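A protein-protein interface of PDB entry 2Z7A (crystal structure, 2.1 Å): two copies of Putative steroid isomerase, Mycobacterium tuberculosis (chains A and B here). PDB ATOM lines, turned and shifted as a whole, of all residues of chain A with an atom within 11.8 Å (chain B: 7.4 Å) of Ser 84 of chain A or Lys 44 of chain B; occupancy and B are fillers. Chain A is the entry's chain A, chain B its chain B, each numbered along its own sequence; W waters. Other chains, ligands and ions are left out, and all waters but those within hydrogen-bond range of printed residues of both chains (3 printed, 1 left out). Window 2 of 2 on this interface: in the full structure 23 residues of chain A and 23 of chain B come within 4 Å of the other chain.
Phe 81 of chain A touches Tyr 127 of chain B.
Pro 82 of chain A touches Asn 129 of chain B (CB to ND2, 3.7 Å).
Ser 83 of chain A touches Ile 42 of chain B (OG to O, 3.6 Å).
Ser 83 of chain A touches Tyr 127 of chain B.
Ser 83 of chain A touches Trp 128 of chain B.
Ser 84 of chain A touches Pro 41 of chain B.
Ser 85 of chain A touches Gly 43 of chain B (N to CA, 3.8 Å).
CG2 of Ile 42 of chain B touches OE2 of Glu 88 of chain A (3.5 Å).
Ile 89 of chain A touches Tyr 127 of chain B.
Tyr 127 of chain B touches Ala 90 of chain A.
The backbone carbonyl oxygen (O) of Glu 88 of chain A is in hydrogen-bond range of the side-chain hydroxyl (OG) of Ser 83 of chain A, 3.0 Å away.
The side-chain hydroxyl (OG) of Ser 85 of chain A sits close to the backbone NH (N) of Asp 87 of chain A (3.0 Å).
The side-chain sulfur (SD) of Met 132 of chain B is in hydrogen-bond range of the backbone NH (N) of Asn 129 of chain B, at 3.5 Å.
The side-chain amide nitrogen of Asn 48 of chain B is in hydrogen-bond range of the backbone carbonyl oxygen of Pro 41 of chain B (2.7 Å).
OG of Ser 83 of chain A sits at hydrogen-bond distance from N of Ser 85 of chain A (2.9 Å).
The backbone NH (N) of Ile 42 of chain B lies within hydrogen-bond range of the backbone carbonyl oxygen (O) of Gly 126 of chain B (2.8 Å).
No position is printed for both chains.
Of the 19 printed residues of chain B, 8 touch a printed residue of chain A.
Hydrophobic or aromatic side chains of chain B within 4 Å of the printed part of chain A: Pro 41, Ile 42, Tyr 127 and Met 132.
Hydrophobic or aromatic side chains of chain A that line the printed part of chain B: Phe 81, Pro 82 and Ala 90.
Among the printed residues, 21 pairs touch across the chains.
Among the printed residues, no Asp or Glu carboxylate lies within 4 Å of a Lys or Arg side-chain nitrogen of the other chain.
The backbone carbonyl oxygen (O) of Ser 83 of chain A is in hydrogen-bond range of the side-chain amide nitrogen (ND2) of Asn 129 of chain B, at 3.0 Å.
The backbone carbonyl oxygen of Trp 128 of chain B sits at hydrogen-bond distance from the side-chain hydroxyl of Ser 84 of chain A, 3.2 Å away.
The backbone NH (N) of Ser 85 of chain A sits at hydrogen-bond distance from the backbone carbonyl oxygen (O) of Ile 42 of chain B (3.3 Å).
The backbone NH (N) of Ser 84 of chain A lies within hydrogen-bond range of the backbone carbonyl oxygen (O) of Ile 42 of chain B, at 2.8 Å.
The backbone carbonyl oxygen (O) of Pro 82 of chain A sits at hydrogen-bond distance from the backbone NH (N) of Trp 128 of chain B (3.2 Å).
The backbone carbonyl oxygen of Pro 82 of chain A sits close to the side-chain sulfur of Met 132 of chain B (3.7 Å).
Water W1 lies within hydrogen-bond range of OE1 of Glu 88 of chain A (2.6 Å), OH of Tyr 127 of chain B (2.7 Å) and O of Tyr 113 of chain A (3.1 Å).
Water W3 bridges O of Lys 44 of chain B (2.7 Å) and O of Ser 84 of chain A (3.1 Å).
Water W2 bridges the side-chain hydroxyl of Ser 84 of chain A (2.7 Å) and the side-chain hydroxyl of Ser 45 of chain B (3.0 Å).
Of the printed residues of chain B, Phe 81 of chain A touches Tyr 127 and Met 132.
Of the printed residues of chain B, Pro 82 of chain A touches Tyr 127 (3.2 Å), Trp 128 (3.2 Å), Asn 129 (3.7 Å) and Met 132 (3.7 Å).
Printed residues of chain B within 4 Å of Glu 88 of chain A: Ile 42.
Of the printed residues of chain B, Ile 89 of chain A touches Tyr 127.
Of the printed residues of chain B, Ala 90 of chain A touches Tyr 127.
Of chain A, only Ser 83, Ser 84, Ser 85 and Glu 88 come within 4 Å of Ile 42 of chain B.
Thr 47 of chain B touches none of the printed residues of chain A.
No residue of chain A comes within 4 Å of Asn 48 of chain B.
No residue of chain A comes within 4 Å of Pro 49 of chain B.
Ser 52 of chain B touches none of the printed residues of chain A.
Of chain A, only Pro 82 (3.2 Å), Ser 83 (3.3 Å) and Ser 84 (3.2 Å) come within 4 Å of Trp 128 of chain B.
Of chain A, only Pro 82 (3.7 Å), Ser 83 (3.0 Å) and Ser 84 (3.4 Å) come within 4 Å of Asn 129 of chain B.
The nearest printed residue of chain B that does not touch Ile 89 of chain A is Ile 42 of chain B (6.4 Å).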
ATOM      1  N   SER A   7     -35.723  -5.033 -30.700  1.00  0.00           N
ATOM      2  CA  SER A   7     -35.156  -5.490 -29.387  1.00  0.00           C
ATOM      3  C   SER A   7     -36.261  -5.613 -28.351  1.00  0.00           C
ATOM      4  O   SER A   7     -37.319  -5.060 -28.548  1.00  0.00           O
ATOM      5  CB  SER A   7     -34.051  -4.578 -28.891  1.00  0.00           C
ATOM      6  OG  SER A   7     -34.539  -3.269 -28.627  1.00  0.00           O
ATOM      7  N   PRO A   8     -36.034  -6.364 -27.273  1.00  0.00           N
ATOM      8  CA  PRO A   8     -36.970  -6.311 -26.148  1.00  0.00           C
ATOM      9  C   PRO A   8     -37.188  -4.903 -25.605  1.00  0.00           C
ATOM     10  O   PRO A   8     -38.306  -4.521 -25.334  1.00  0.00           O
ATOM     11  CB  PRO A   8     -36.296  -7.203 -25.139  1.00  0.00           C
ATOM     12  CG  PRO A   8     -35.575  -8.153 -25.893  1.00  0.00           C
ATOM     13  CD  PRO A   8     -34.959  -7.322 -26.984  1.00  0.00           C
ATOM     14  N   ALA A   9     -36.132  -4.092 -25.488  1.00  0.00           N
ATOM     15  CA  ALA A   9     -36.312  -2.738 -24.967  1.00  0.00           C
ATOM     16  C   ALA A   9     -37.164  -1.935 -25.922  1.00  0.00           C
ATOM     17  O   ALA A   9     -37.979  -1.092 -25.497  1.00  0.00           O
ATOM     18  CB  ALA A   9     -34.956  -2.047 -24.728  1.00  0.00           C
ATOM     19  N   LEU A  10     -36.958  -2.121 -27.226  1.00  0.00           N
ATOM     20  CA  LEU A  10     -37.749  -1.306 -28.186  1.00  0.00           C
ATOM     21  C   LEU A  10     -39.267  -1.748 -28.239  1.00  0.00           C
ATOM     22  O   LEU A  10     -40.170  -0.945 -28.234  1.00  0.00           O
ATOM     23  CB  LEU A  10     -37.087  -1.283 -29.592  1.00  0.00           C
ATOM     24  CG  LEU A  10     -37.937  -0.514 -30.642  1.00  0.00           C
ATOM     25  CD1 LEU A  10     -37.995   0.975 -30.354  1.00  0.00           C
ATOM     26  CD2 LEU A  10     -37.436  -0.739 -32.103  1.00  0.00           C
ATOM     27  N   THR A  80     -35.124   7.931 -31.517  1.00  0.00           N
ATOM     28  CA  THR A  80     -34.722   6.806 -30.687  1.00  0.00           C
ATOM     29  C   THR A  80     -33.198   6.590 -30.707  1.00  0.00           C
ATOM     30  O   THR A  80     -32.573   6.623 -31.786  1.00  0.00           O
ATOM     31  CB  THR A  80     -35.362   5.567 -31.211  1.00  0.00           C
ATOM     32  OG1 THR A  80     -36.776   5.706 -31.091  1.00  0.00           O
ATOM     33  CG2 THR A  80     -34.936   4.324 -30.432  1.00  0.00           C
ATOM     34  N   PHE A  81     -32.637   6.292 -29.526  1.00  0.00           N
ATOM     35  CA  PHE A  81     -31.214   5.969 -29.382  1.00  0.00           C
ATOM     36  C   PHE A  81     -31.011   4.583 -28.792  1.00  0.00           C
ATOM     37  O   PHE A  81     -31.047   4.435 -27.556  1.00  0.00           O
ATOM     38  CB  PHE A  81     -30.541   7.037 -28.508  1.00  0.00           C
ATOM     39  CG  PHE A  81     -30.534   8.394 -29.147  1.00  0.00           C
ATOM     40  CD1 PHE A  81     -29.424   8.852 -29.866  1.00  0.00           C
ATOM     41  CD2 PHE A  81     -31.641   9.221 -29.017  1.00  0.00           C
ATOM     42  CE1 PHE A  81     -29.445  10.104 -30.455  1.00  0.00           C
ATOM     43  CE2 PHE A  81     -31.657  10.473 -29.614  1.00  0.00           C
ATOM     44  CZ  PHE A  81     -30.537  10.909 -30.323  1.00  0.00           C
ATOM     45  N   PRO A  82     -30.819   3.551 -29.653  1.00  0.00           N
ATOM     46  CA  PRO A  82     -30.552   2.205 -29.158  1.00  0.00           C
ATOM     47  C   PRO A  82     -29.189   2.269 -28.417  1.00  0.00           C
ATOM     48  O   PRO A  82     -28.426   3.182 -28.667  1.00  0.00           O
ATOM     49  CB  PRO A  82     -30.388   1.388 -30.443  1.00  0.00           C
ATOM     50  CG  PRO A  82     -31.126   2.207 -31.531  1.00  0.00           C
ATOM     51  CD  PRO A  82     -30.823   3.616 -31.140  1.00  0.00           C
ATOM     52  N   SER A  83     -28.923   1.343 -27.511  1.00  0.00           N
ATOM     53  CA  SER A  83     -27.615   1.236 -26.880  1.00  0.00           C
ATOM     54  C   SER A  83     -26.940  -0.028 -27.503  1.00  0.00           C
ATOM     55  O   SER A  83     -27.418  -0.571 -28.525  1.00  0.00           O
ATOM     56  CB  SER A  83     -27.784   1.151 -25.325  1.00  0.00           C
ATOM     57  OG  SER A  83     -28.148  -0.175 -24.934  1.00  0.00           O
ATOM     58  N   SER A  84     -25.885  -0.557 -26.884  1.00  0.00           N
ATOM     59  CA  SER A  84     -25.399  -1.870 -27.327  1.00  0.00           C
ATOM     60  C   SER A  84     -25.991  -3.005 -26.552  1.00  0.00           C
ATOM     61  O   SER A  84     -25.541  -4.165 -26.671  1.00  0.00           O
ATOM     62  CB  SER A  84     -23.873  -1.908 -27.268  1.00  0.00           C
ATOM     63  OG  SER A  84     -23.340  -0.882 -28.084  1.00  0.00           O
ATOM     64  N   SER A  85     -26.955  -2.688 -25.676  1.00  0.00           N
ATOM     65  CA  SER A  85     -27.692  -3.753 -25.004  1.00  0.00           C
ATOM     66  C   SER A  85     -29.104  -3.845 -25.663  1.00  0.00           C
ATOM     67  O   SER A  85     -29.715  -2.824 -25.861  1.00  0.00           O
ATOM     68  CB  SER A  85     -27.849  -3.439 -23.476  1.00  0.00           C
ATOM     69  OG  SER A  85     -28.782  -4.350 -22.884  1.00  0.00           O
ATOM     70  N   PRO A  86     -29.591  -5.050 -26.025  1.00  0.00           N
ATOM     71  CA  PRO A  86     -30.968  -5.131 -26.530  1.00  0.00           C
ATOM     72  C   PRO A  86     -31.988  -4.781 -25.415  1.00  0.00           C
ATOM     73  O   PRO A  86     -33.168  -4.689 -25.706  1.00  0.00           O
ATOM     74  CB  PRO A  86     -31.176  -6.617 -26.831  1.00  0.00           C
ATOM     75  CG  PRO A  86     -29.990  -7.343 -26.256  1.00  0.00           C
ATOM     76  CD  PRO A  86     -28.888  -6.358 -26.035  1.00  0.00           C
ATOM     77  N   ASP A  87     -31.505  -4.609 -24.174  1.00  0.00           N
ATOM     78  CA  ASP A  87     -32.353  -4.499 -23.026  1.00  0.00           C
ATOM     79  C   ASP A  87     -32.467  -3.097 -22.494  1.00  0.00           C
ATOM     80  O   ASP A  87     -33.179  -2.877 -21.509  1.00  0.00           O
ATOM     81  CB  ASP A  87     -31.901  -5.432 -21.919  1.00  0.00           C
ATOM     82  CG  ASP A  87     -32.152  -6.902 -22.223  1.00  0.00           C
ATOM     83  OD1 ASP A  87     -32.882  -7.281 -23.173  1.00  0.00           O
ATOM     84  OD2 ASP A  87     -31.673  -7.711 -21.411  1.00  0.00           O
ATOM     85  N   GLU A  88     -31.795  -2.136 -23.121  1.00  0.00           N
ATOM     86  CA  GLU A  88     -31.864  -0.721 -22.676  1.00  0.00           C
ATOM     87  C   GLU A  88     -31.877   0.223 -23.847  1.00  0.00           C
ATOM     88  O   GLU A  88     -31.120  -0.003 -24.793  1.00  0.00           O
ATOM     89  CB  GLU A  88     -30.637  -0.363 -21.796  1.00  0.00           C
ATOM     90  CG  GLU A  88     -30.592  -1.234 -20.518  1.00  0.00           C
ATOM     91  CD  GLU A  88     -29.828  -0.584 -19.418  1.00  0.00           C
ATOM     92  OE1 GLU A  88     -30.098   0.588 -18.984  1.00  0.00           O
ATOM     93  OE2 GLU A  88     -28.953  -1.285 -18.973  1.00  0.00           O
ATOM     94  N   ILE A  89     -32.688   1.282 -23.763  1.00  0.00           N
ATOM     95  CA  ILE A  89     -32.930   2.169 -24.872  1.00  0.00           C
ATOM     96  C   ILE A  89     -33.274   3.521 -24.346  1.00  0.00           C
ATOM     97  O   ILE A  89     -33.785   3.650 -23.212  1.00  0.00           O
ATOM     98  CB  ILE A  89     -34.113   1.548 -25.798  1.00  0.00           C
ATOM     99  CG1 ILE A  89     -34.156   2.191 -27.148  1.00  0.00           C
ATOM    100  CG2 ILE A  89     -35.475   1.695 -25.122  1.00  0.00           C
ATOM    101  CD1 ILE A  89     -34.844   1.279 -28.304  1.00  0.00           C
ATOM    102  N   ALA A  90     -32.971   4.565 -25.122  1.00  0.00           N
ATOM    103  CA  ALA A  90     -33.389   5.922 -24.825  1.00  0.00           C
ATOM    104  C   ALA A  90     -34.215   6.483 -25.992  1.00  0.00           C
ATOM    105  O   ALA A  90     -34.013   6.077 -27.143  1.00  0.00           O
ATOM    106  CB  ALA A  90     -32.218   6.813 -24.589  1.00  0.00           C
ATOM    107  N   TYR A 113     -35.438   3.337 -20.893  1.00  0.00           N
ATOM    108  CA  TYR A 113     -36.195   2.188 -20.479  1.00  0.00           C
ATOM    109  C   TYR A 113     -35.213   1.082 -20.314  1.00  0.00           C
ATOM    110  O   TYR A 113     -34.342   0.952 -21.179  1.00  0.00           O
ATOM    111  CB  TYR A 113     -37.199   1.759 -21.597  1.00  0.00           C
ATOM    112  CG  TYR A 113     -38.286   2.742 -21.871  1.00  0.00           C
ATOM    113  CD1 TYR A 113     -39.617   2.436 -21.565  1.00  0.00           C
ATOM    114  CD2 TYR A 113     -38.012   3.943 -22.468  1.00  0.00           C
ATOM    115  CE1 TYR A 113     -40.618   3.332 -21.812  1.00  0.00           C
ATOM    116  CE2 TYR A 113     -39.014   4.834 -22.718  1.00  0.00           C
ATOM    117  CZ  TYR A 113     -40.304   4.546 -22.386  1.00  0.00           C
ATOM    118  OH  TYR A 113     -41.297   5.507 -22.688  1.00  0.00           O
ATOM    119  N   ARG A 114     -35.343   0.295 -19.250  1.00  0.00           N
ATOM    120  CA  ARG A 114     -34.630  -0.943 -19.136  1.00  0.00           C
ATOM    121  C   ARG A 114     -35.580  -2.116 -18.887  1.00  0.00           C
ATOM    122  O   ARG A 114     -36.536  -2.044 -18.051  1.00  0.00           O
ATOM    123  CB  ARG A 114     -33.636  -0.887 -17.906  1.00  0.00           C
ATOM    124  CG  ARG A 114     -32.969  -2.239 -17.658  1.00  0.00           C
ATOM    125  CD  ARG A 114     -32.070  -2.206 -16.377  1.00  0.00           C
ATOM    126  NE  ARG A 114     -31.343  -3.469 -16.266  1.00  0.00           N
ATOM    127  CZ  ARG A 114     -31.799  -4.587 -15.673  1.00  0.00           C
ATOM    128  NH1 ARG A 114     -33.045  -4.694 -15.172  1.00  0.00           N
ATOM    129  NH2 ARG A 114     -31.010  -5.641 -15.635  1.00  0.00           N
ATOM    130  N   VAL A 115     -35.285  -3.236 -19.518  1.00  0.00           N
ATOM    131  CA  VAL A 115     -36.039  -4.445 -19.288  1.00  0.00           C
ATOM    132  C   VAL A 115     -35.198  -5.549 -18.680  1.00  0.00           C
ATOM    133  O   VAL A 115     -33.985  -5.565 -18.931  1.00  0.00           O
ATOM    134  CB  VAL A 115     -36.789  -4.981 -20.602  1.00  0.00           C
ATOM    135  CG1 VAL A 115     -37.731  -3.940 -21.162  1.00  0.00           C
ATOM    136  CG2 VAL A 115     -35.841  -5.457 -21.680  1.00  0.00           C
ATOM    137  N   ASP B  40     -19.966   3.124 -21.477  1.00  0.00           N
ATOM    138  CA  ASP B  40     -19.904   3.901 -22.696  1.00  0.00           C
ATOM    139  C   ASP B  40     -19.442   3.030 -23.877  1.00  0.00           C
ATOM    140  O   ASP B  40     -18.219   2.919 -24.079  1.00  0.00           O
ATOM    141  CB  ASP B  40     -18.959   5.110 -22.436  1.00  0.00           C
ATOM    142  CG  ASP B  40     -18.891   6.101 -23.623  1.00  0.00           C
ATOM    143  OD1 ASP B  40     -19.812   6.069 -24.489  1.00  0.00           O
ATOM    144  OD2 ASP B  40     -17.925   6.919 -23.657  1.00  0.00           O
ATOM    145  N   PRO B  41     -20.384   2.352 -24.616  1.00  0.00           N
ATOM    146  CA  PRO B  41     -21.872   2.455 -24.458  1.00  0.00           C
ATOM    147  C   PRO B  41     -22.420   1.444 -23.433  1.00  0.00           C
ATOM    148  O   PRO B  41     -21.661   0.580 -22.892  1.00  0.00           O
ATOM    149  CB  PRO B  41     -22.412   2.104 -25.866  1.00  0.00           C
ATOM    150  CG  PRO B  41     -21.447   1.009 -26.365  1.00  0.00           C
ATOM    151  CD  PRO B  41     -20.044   1.299 -25.587  1.00  0.00           C
ATOM    152  N   ILE B  42     -23.731   1.517 -23.155  1.00  0.00           N
ATOM    153  CA  ILE B  42     -24.344   0.492 -22.326  1.00  0.00           C
ATOM    154  C   ILE B  42     -24.366  -0.761 -23.194  1.00  0.00           C
ATOM    155  O   ILE B  42     -24.619  -0.678 -24.403  1.00  0.00           O
ATOM    156  CB  ILE B  42     -25.814   0.938 -21.946  1.00  0.00           C
ATOM    157  CG1 ILE B  42     -25.772   2.231 -21.130  1.00  0.00           C
ATOM    158  CG2 ILE B  42     -26.616  -0.253 -21.332  1.00  0.00           C
ATOM    159  CD1 ILE B  42     -27.171   3.061 -21.149  1.00  0.00           C
ATOM    160  N   GLY B  43     -23.980  -1.892 -22.618  1.00  0.00           N
ATOM    161  CA  GLY B  43     -23.975  -3.131 -23.350  1.00  0.00           C
ATOM    162  C   GLY B  43     -22.597  -3.559 -23.810  1.00  0.00           C
ATOM    163  O   GLY B  43     -21.699  -2.729 -23.907  1.00  0.00           O
ATOM    164  N   LYS B  44     -22.474  -4.839 -24.157  1.00  0.00           N
ATOM    165  CA  LYS B  44     -21.208  -5.427 -24.584  1.00  0.00           C
ATOM    166  C   LYS B  44     -20.620  -4.734 -25.804  1.00  0.00           C
ATOM    167  O   LYS B  44     -21.232  -4.720 -26.865  1.00  0.00           O
ATOM    168  CB  LYS B  44     -21.364  -6.935 -24.836  1.00  0.00           C
ATOM    169  CG  LYS B  44     -20.013  -7.687 -24.806  1.00  0.00           C
ATOM    170  CD  LYS B  44     -20.106  -9.189 -25.159  1.00  0.00           C
ATOM    171  CE  LYS B  44     -18.712  -9.822 -25.003  1.00  0.00           C
ATOM    172  NZ  LYS B  44     -18.342 -10.162 -23.588  1.00  0.00           N
ATOM    173  N   SER B  45     -19.434  -4.148 -25.636  1.00  0.00           N
ATOM    174  CA  SER B  45     -18.704  -3.457 -26.722  1.00  0.00           C
ATOM    175  C   SER B  45     -17.187  -3.476 -26.389  1.00  0.00           C
ATOM    176  O   SER B  45     -16.822  -3.898 -25.299  1.00  0.00           O
ATOM    177  CB  SER B  45     -19.191  -2.003 -26.886  1.00  0.00           C
ATOM    178  OG  SER B  45     -18.878  -1.464 -28.206  1.00  0.00           O
ATOM    179  N   VAL B  46     -16.341  -2.991 -27.304  1.00  0.00           N
ATOM    180  CA  VAL B  46     -14.879  -2.830 -27.081  1.00  0.00           C
ATOM    181  C   VAL B  46     -14.562  -1.959 -25.846  1.00  0.00           C
ATOM    182  O   VAL B  46     -13.635  -2.262 -25.059  1.00  0.00           O
ATOM    183  CB  VAL B  46     -14.193  -2.170 -28.341  1.00  0.00           C
ATOM    184  CG1 VAL B  46     -12.718  -1.875 -28.085  1.00  0.00           C
ATOM    185  CG2 VAL B  46     -14.344  -3.047 -29.623  1.00  0.00           C
ATOM    186  N   THR B  47     -15.346  -0.883 -25.687  1.00  0.00           N
ATOM    187  CA  THR B  47     -15.218   0.097 -24.557  1.00  0.00           C
ATOM    188  C   THR B  47     -16.091  -0.258 -23.319  1.00  0.00           C
ATOM    189  O   THR B  47     -16.048   0.440 -22.273  1.00  0.00           O
ATOM    190  CB  THR B  47     -15.509   1.544 -25.026  1.00  0.00           C
ATOM    191  OG1 THR B  47     -16.789   1.606 -25.673  1.00  0.00           O
ATOM    192  CG2 THR B  47     -14.489   2.000 -26.042  1.00  0.00           C
ATOM    193  N   ASN B  48     -16.847  -1.355 -23.430  1.00  0.00           N
ATOM    194  CA  ASN B  48     -17.596  -1.918 -22.311  1.00  0.00           C
ATOM    195  C   ASN B  48     -17.490  -3.435 -22.425  1.00  0.00           C
ATOM    196  O   ASN B  48     -18.485  -4.103 -22.687  1.00  0.00           O
ATOM    197  CB  ASN B  48     -19.082  -1.427 -22.327  1.00  0.00           C
ATOM    198  CG  ASN B  48     -19.854  -1.739 -21.022  1.00  0.00           C
ATOM    199  OD1 ASN B  48     -19.440  -2.571 -20.173  1.00  0.00           O
ATOM    200  ND2 ASN B  48     -21.002  -1.063 -20.857  1.00  0.00           N
ATOM    201  N   PRO B  49     -16.267  -3.982 -22.236  1.00  0.00           N
ATOM    202  CA  PRO B  49     -16.057  -5.334 -22.732  1.00  0.00           C
ATOM    203  C   PRO B  49     -16.845  -6.453 -22.015  1.00  0.00           C
ATOM    204  O   PRO B  49     -17.047  -7.484 -22.621  1.00  0.00           O
ATOM    205  CB  PRO B  49     -14.524  -5.505 -22.630  1.00  0.00           C
ATOM    206  CG  PRO B  49     -14.125  -4.618 -21.515  1.00  0.00           C
ATOM    207  CD  PRO B  49     -15.022  -3.428 -21.623  1.00  0.00           C
ATOM    208  N   ASP B  50     -17.306  -6.246 -20.782  1.00  0.00           N
ATOM    209  CA  ASP B  50     -18.177  -7.242 -20.117  1.00  0.00           C
ATOM    210  C   ASP B  50     -19.688  -6.899 -20.123  1.00  0.00           C
ATOM    211  O   ASP B  50     -20.494  -7.662 -19.581  1.00  0.00           O
ATOM    212  CB  ASP B  50     -17.607  -7.712 -18.734  1.00  0.00           C
ATOM    213  CG  ASP B  50     -18.093  -6.877 -17.512  1.00  0.00           C
ATOM    214  OD1 ASP B  50     -18.706  -5.783 -17.635  1.00  0.00           O
ATOM    215  OD2 ASP B  50     -17.830  -7.339 -16.370  1.00  0.00           O
ATOM    216  N   GLY B  51     -20.057  -5.778 -20.766  1.00  0.00           N
ATOM    217  CA  GLY B  51     -21.423  -5.322 -20.821  1.00  0.00           C
ATOM    218  C   GLY B  51     -22.008  -4.862 -19.512  1.00  0.00           C
ATOM    219  O   GLY B  51     -23.182  -4.541 -19.441  1.00  0.00           O
ATOM    220  N   SER B  52     -21.205  -4.786 -18.458  1.00  0.00           N
ATOM    221  CA  SER B  52     -21.723  -4.286 -17.182  1.00  0.00           C
ATOM    222  C   SER B  52     -21.004  -3.044 -16.627  1.00  0.00           C
ATOM    223  O   SER B  52     -21.253  -2.604 -15.480  1.00  0.00           O
ATOM    224  CB  SER B  52     -21.738  -5.416 -16.146  1.00  0.00           C
ATOM    225  OG  SER B  52     -20.411  -5.876 -15.958  1.00  0.00           O
ATOM    226  N   GLY B 126     -23.985   5.533 -21.914  1.00  0.00           N
ATOM    227  CA  GLY B 126     -24.094   6.002 -23.338  1.00  0.00           C
ATOM    228  C   GLY B 126     -25.026   5.136 -24.137  1.00  0.00           C
ATOM    229  O   GLY B 126     -24.818   3.910 -24.203  1.00  0.00           O
ATOM    230  N   TYR B 127     -26.045   5.753 -24.746  1.00  0.00           N
ATOM    231  CA  TYR B 127     -27.008   5.007 -25.622  1.00  0.00           C
ATOM    232  C   TYR B 127     -26.508   5.191 -27.049  1.00  0.00           C
ATOM    233  O   TYR B 127     -26.787   6.177 -27.694  1.00  0.00           O
ATOM    234  CB  TYR B 127     -28.485   5.550 -25.447  1.00  0.00           C
ATOM    235  CG  TYR B 127     -28.994   5.251 -24.050  1.00  0.00           C
ATOM    236  CD1 TYR B 127     -29.831   4.155 -23.822  1.00  0.00           C
ATOM    237  CD2 TYR B 127     -28.596   6.061 -22.959  1.00  0.00           C
ATOM    238  CE1 TYR B 127     -30.300   3.880 -22.508  1.00  0.00           C
ATOM    239  CE2 TYR B 127     -29.056   5.812 -21.648  1.00  0.00           C
ATOM    240  CZ  TYR B 127     -29.875   4.709 -21.433  1.00  0.00           C
ATOM    241  OH  TYR B 127     -30.321   4.420 -20.124  1.00  0.00           O
ATOM    242  N   TRP B 128     -25.646   4.281 -27.470  1.00  0.00           N
ATOM    243  CA  TRP B 128     -25.150   4.266 -28.864  1.00  0.00           C
ATOM    244  C   TRP B 128     -24.647   2.883 -29.118  1.00  0.00           C
ATOM    245  O   TRP B 128     -24.519   2.049 -28.214  1.00  0.00           O
ATOM    246  CB  TRP B 128     -24.139   5.412 -29.240  1.00  0.00           C
ATOM    247  CG  TRP B 128     -22.785   5.286 -28.463  1.00  0.00           C
ATOM    248  CD1 TRP B 128     -22.466   5.829 -27.207  1.00  0.00           C
ATOM    249  CD2 TRP B 128     -21.645   4.536 -28.876  1.00  0.00           C
ATOM    250  NE1 TRP B 128     -21.196   5.426 -26.841  1.00  0.00           N
ATOM    251  CE2 TRP B 128     -20.661   4.662 -27.859  1.00  0.00           C
ATOM    252  CE3 TRP B 128     -21.346   3.776 -30.020  1.00  0.00           C
ATOM    253  CZ2 TRP B 128     -19.405   4.054 -27.962  1.00  0.00           C
ATOM    254  CZ3 TRP B 128     -20.082   3.179 -30.115  1.00  0.00           C
ATOM    255  CH2 TRP B 128     -19.128   3.353 -29.092  1.00  0.00           C
ATOM    256  N   ASN B 129     -24.531   2.582 -30.392  1.00  0.00           N
ATOM    257  CA  ASN B 129     -23.797   1.402 -30.863  1.00  0.00           C
ATOM    258  C   ASN B 129     -23.088   1.711 -32.208  1.00  0.00           C
ATOM    259  O   ASN B 129     -23.071   2.858 -32.699  1.00  0.00           O
ATOM    260  CB  ASN B 129     -24.730   0.161 -30.963  1.00  0.00           C
ATOM    261  CG  ASN B 129     -25.860   0.379 -31.874  1.00  0.00           C
ATOM    262  OD1 ASN B 129     -25.676   0.872 -32.974  1.00  0.00           O
ATOM    263  ND2 ASN B 129     -27.053   0.058 -31.435  1.00  0.00           N
ATOM    264  N   LEU B 130     -22.488   0.676 -32.762  1.00  0.00           N
ATOM    265  CA  LEU B 130     -21.704   0.786 -33.994  1.00  0.00           C
ATOM    266  C   LEU B 130     -22.497   1.203 -35.224  1.00  0.00           C
ATOM    267  O   LEU B 130     -21.986   1.986 -36.046  1.00  0.00           O
ATOM    268  CB  LEU B 130     -20.921  -0.508 -34.240  1.00  0.00           C
ATOM    269  CG  LEU B 130     -19.754  -0.764 -33.286  1.00  0.00           C
ATOM    270  CD1 LEU B 130     -18.928  -1.848 -33.934  1.00  0.00           C
ATOM    271  CD2 LEU B 130     -18.881   0.495 -32.975  1.00  0.00           C
ATOM    272  N   MET B 132     -24.432   3.315 -35.262  1.00  0.00           N
ATOM    273  CA  MET B 132     -24.609   4.749 -35.224  1.00  0.00           C
ATOM    274  C   MET B 132     -23.310   5.536 -35.512  1.00  0.00           C
ATOM    275  O   MET B 132     -23.295   6.784 -35.502  1.00  0.00           O
ATOM    276  CB  MET B 132     -25.254   5.149 -33.875  1.00  0.00           C
ATOM    277  CG  MET B 132     -26.603   4.409 -33.672  1.00  0.00           C
ATOM    278  SD  MET B 132     -27.141   4.360 -31.969  1.00  0.00           S
ATOM    279  CE  MET B 132     -27.425   6.068 -31.596  1.00  0.00           C
HETATM  280  O   HOH W   1     -31.980   2.299 -19.706  1.00  0.00           O
HETATM  281  O   HOH W   2     -21.374  -1.336 -29.931  1.00  0.00           O
HETATM  282  O   HOH W   3     -23.333  -5.814 -28.084  1.00  0.00           O
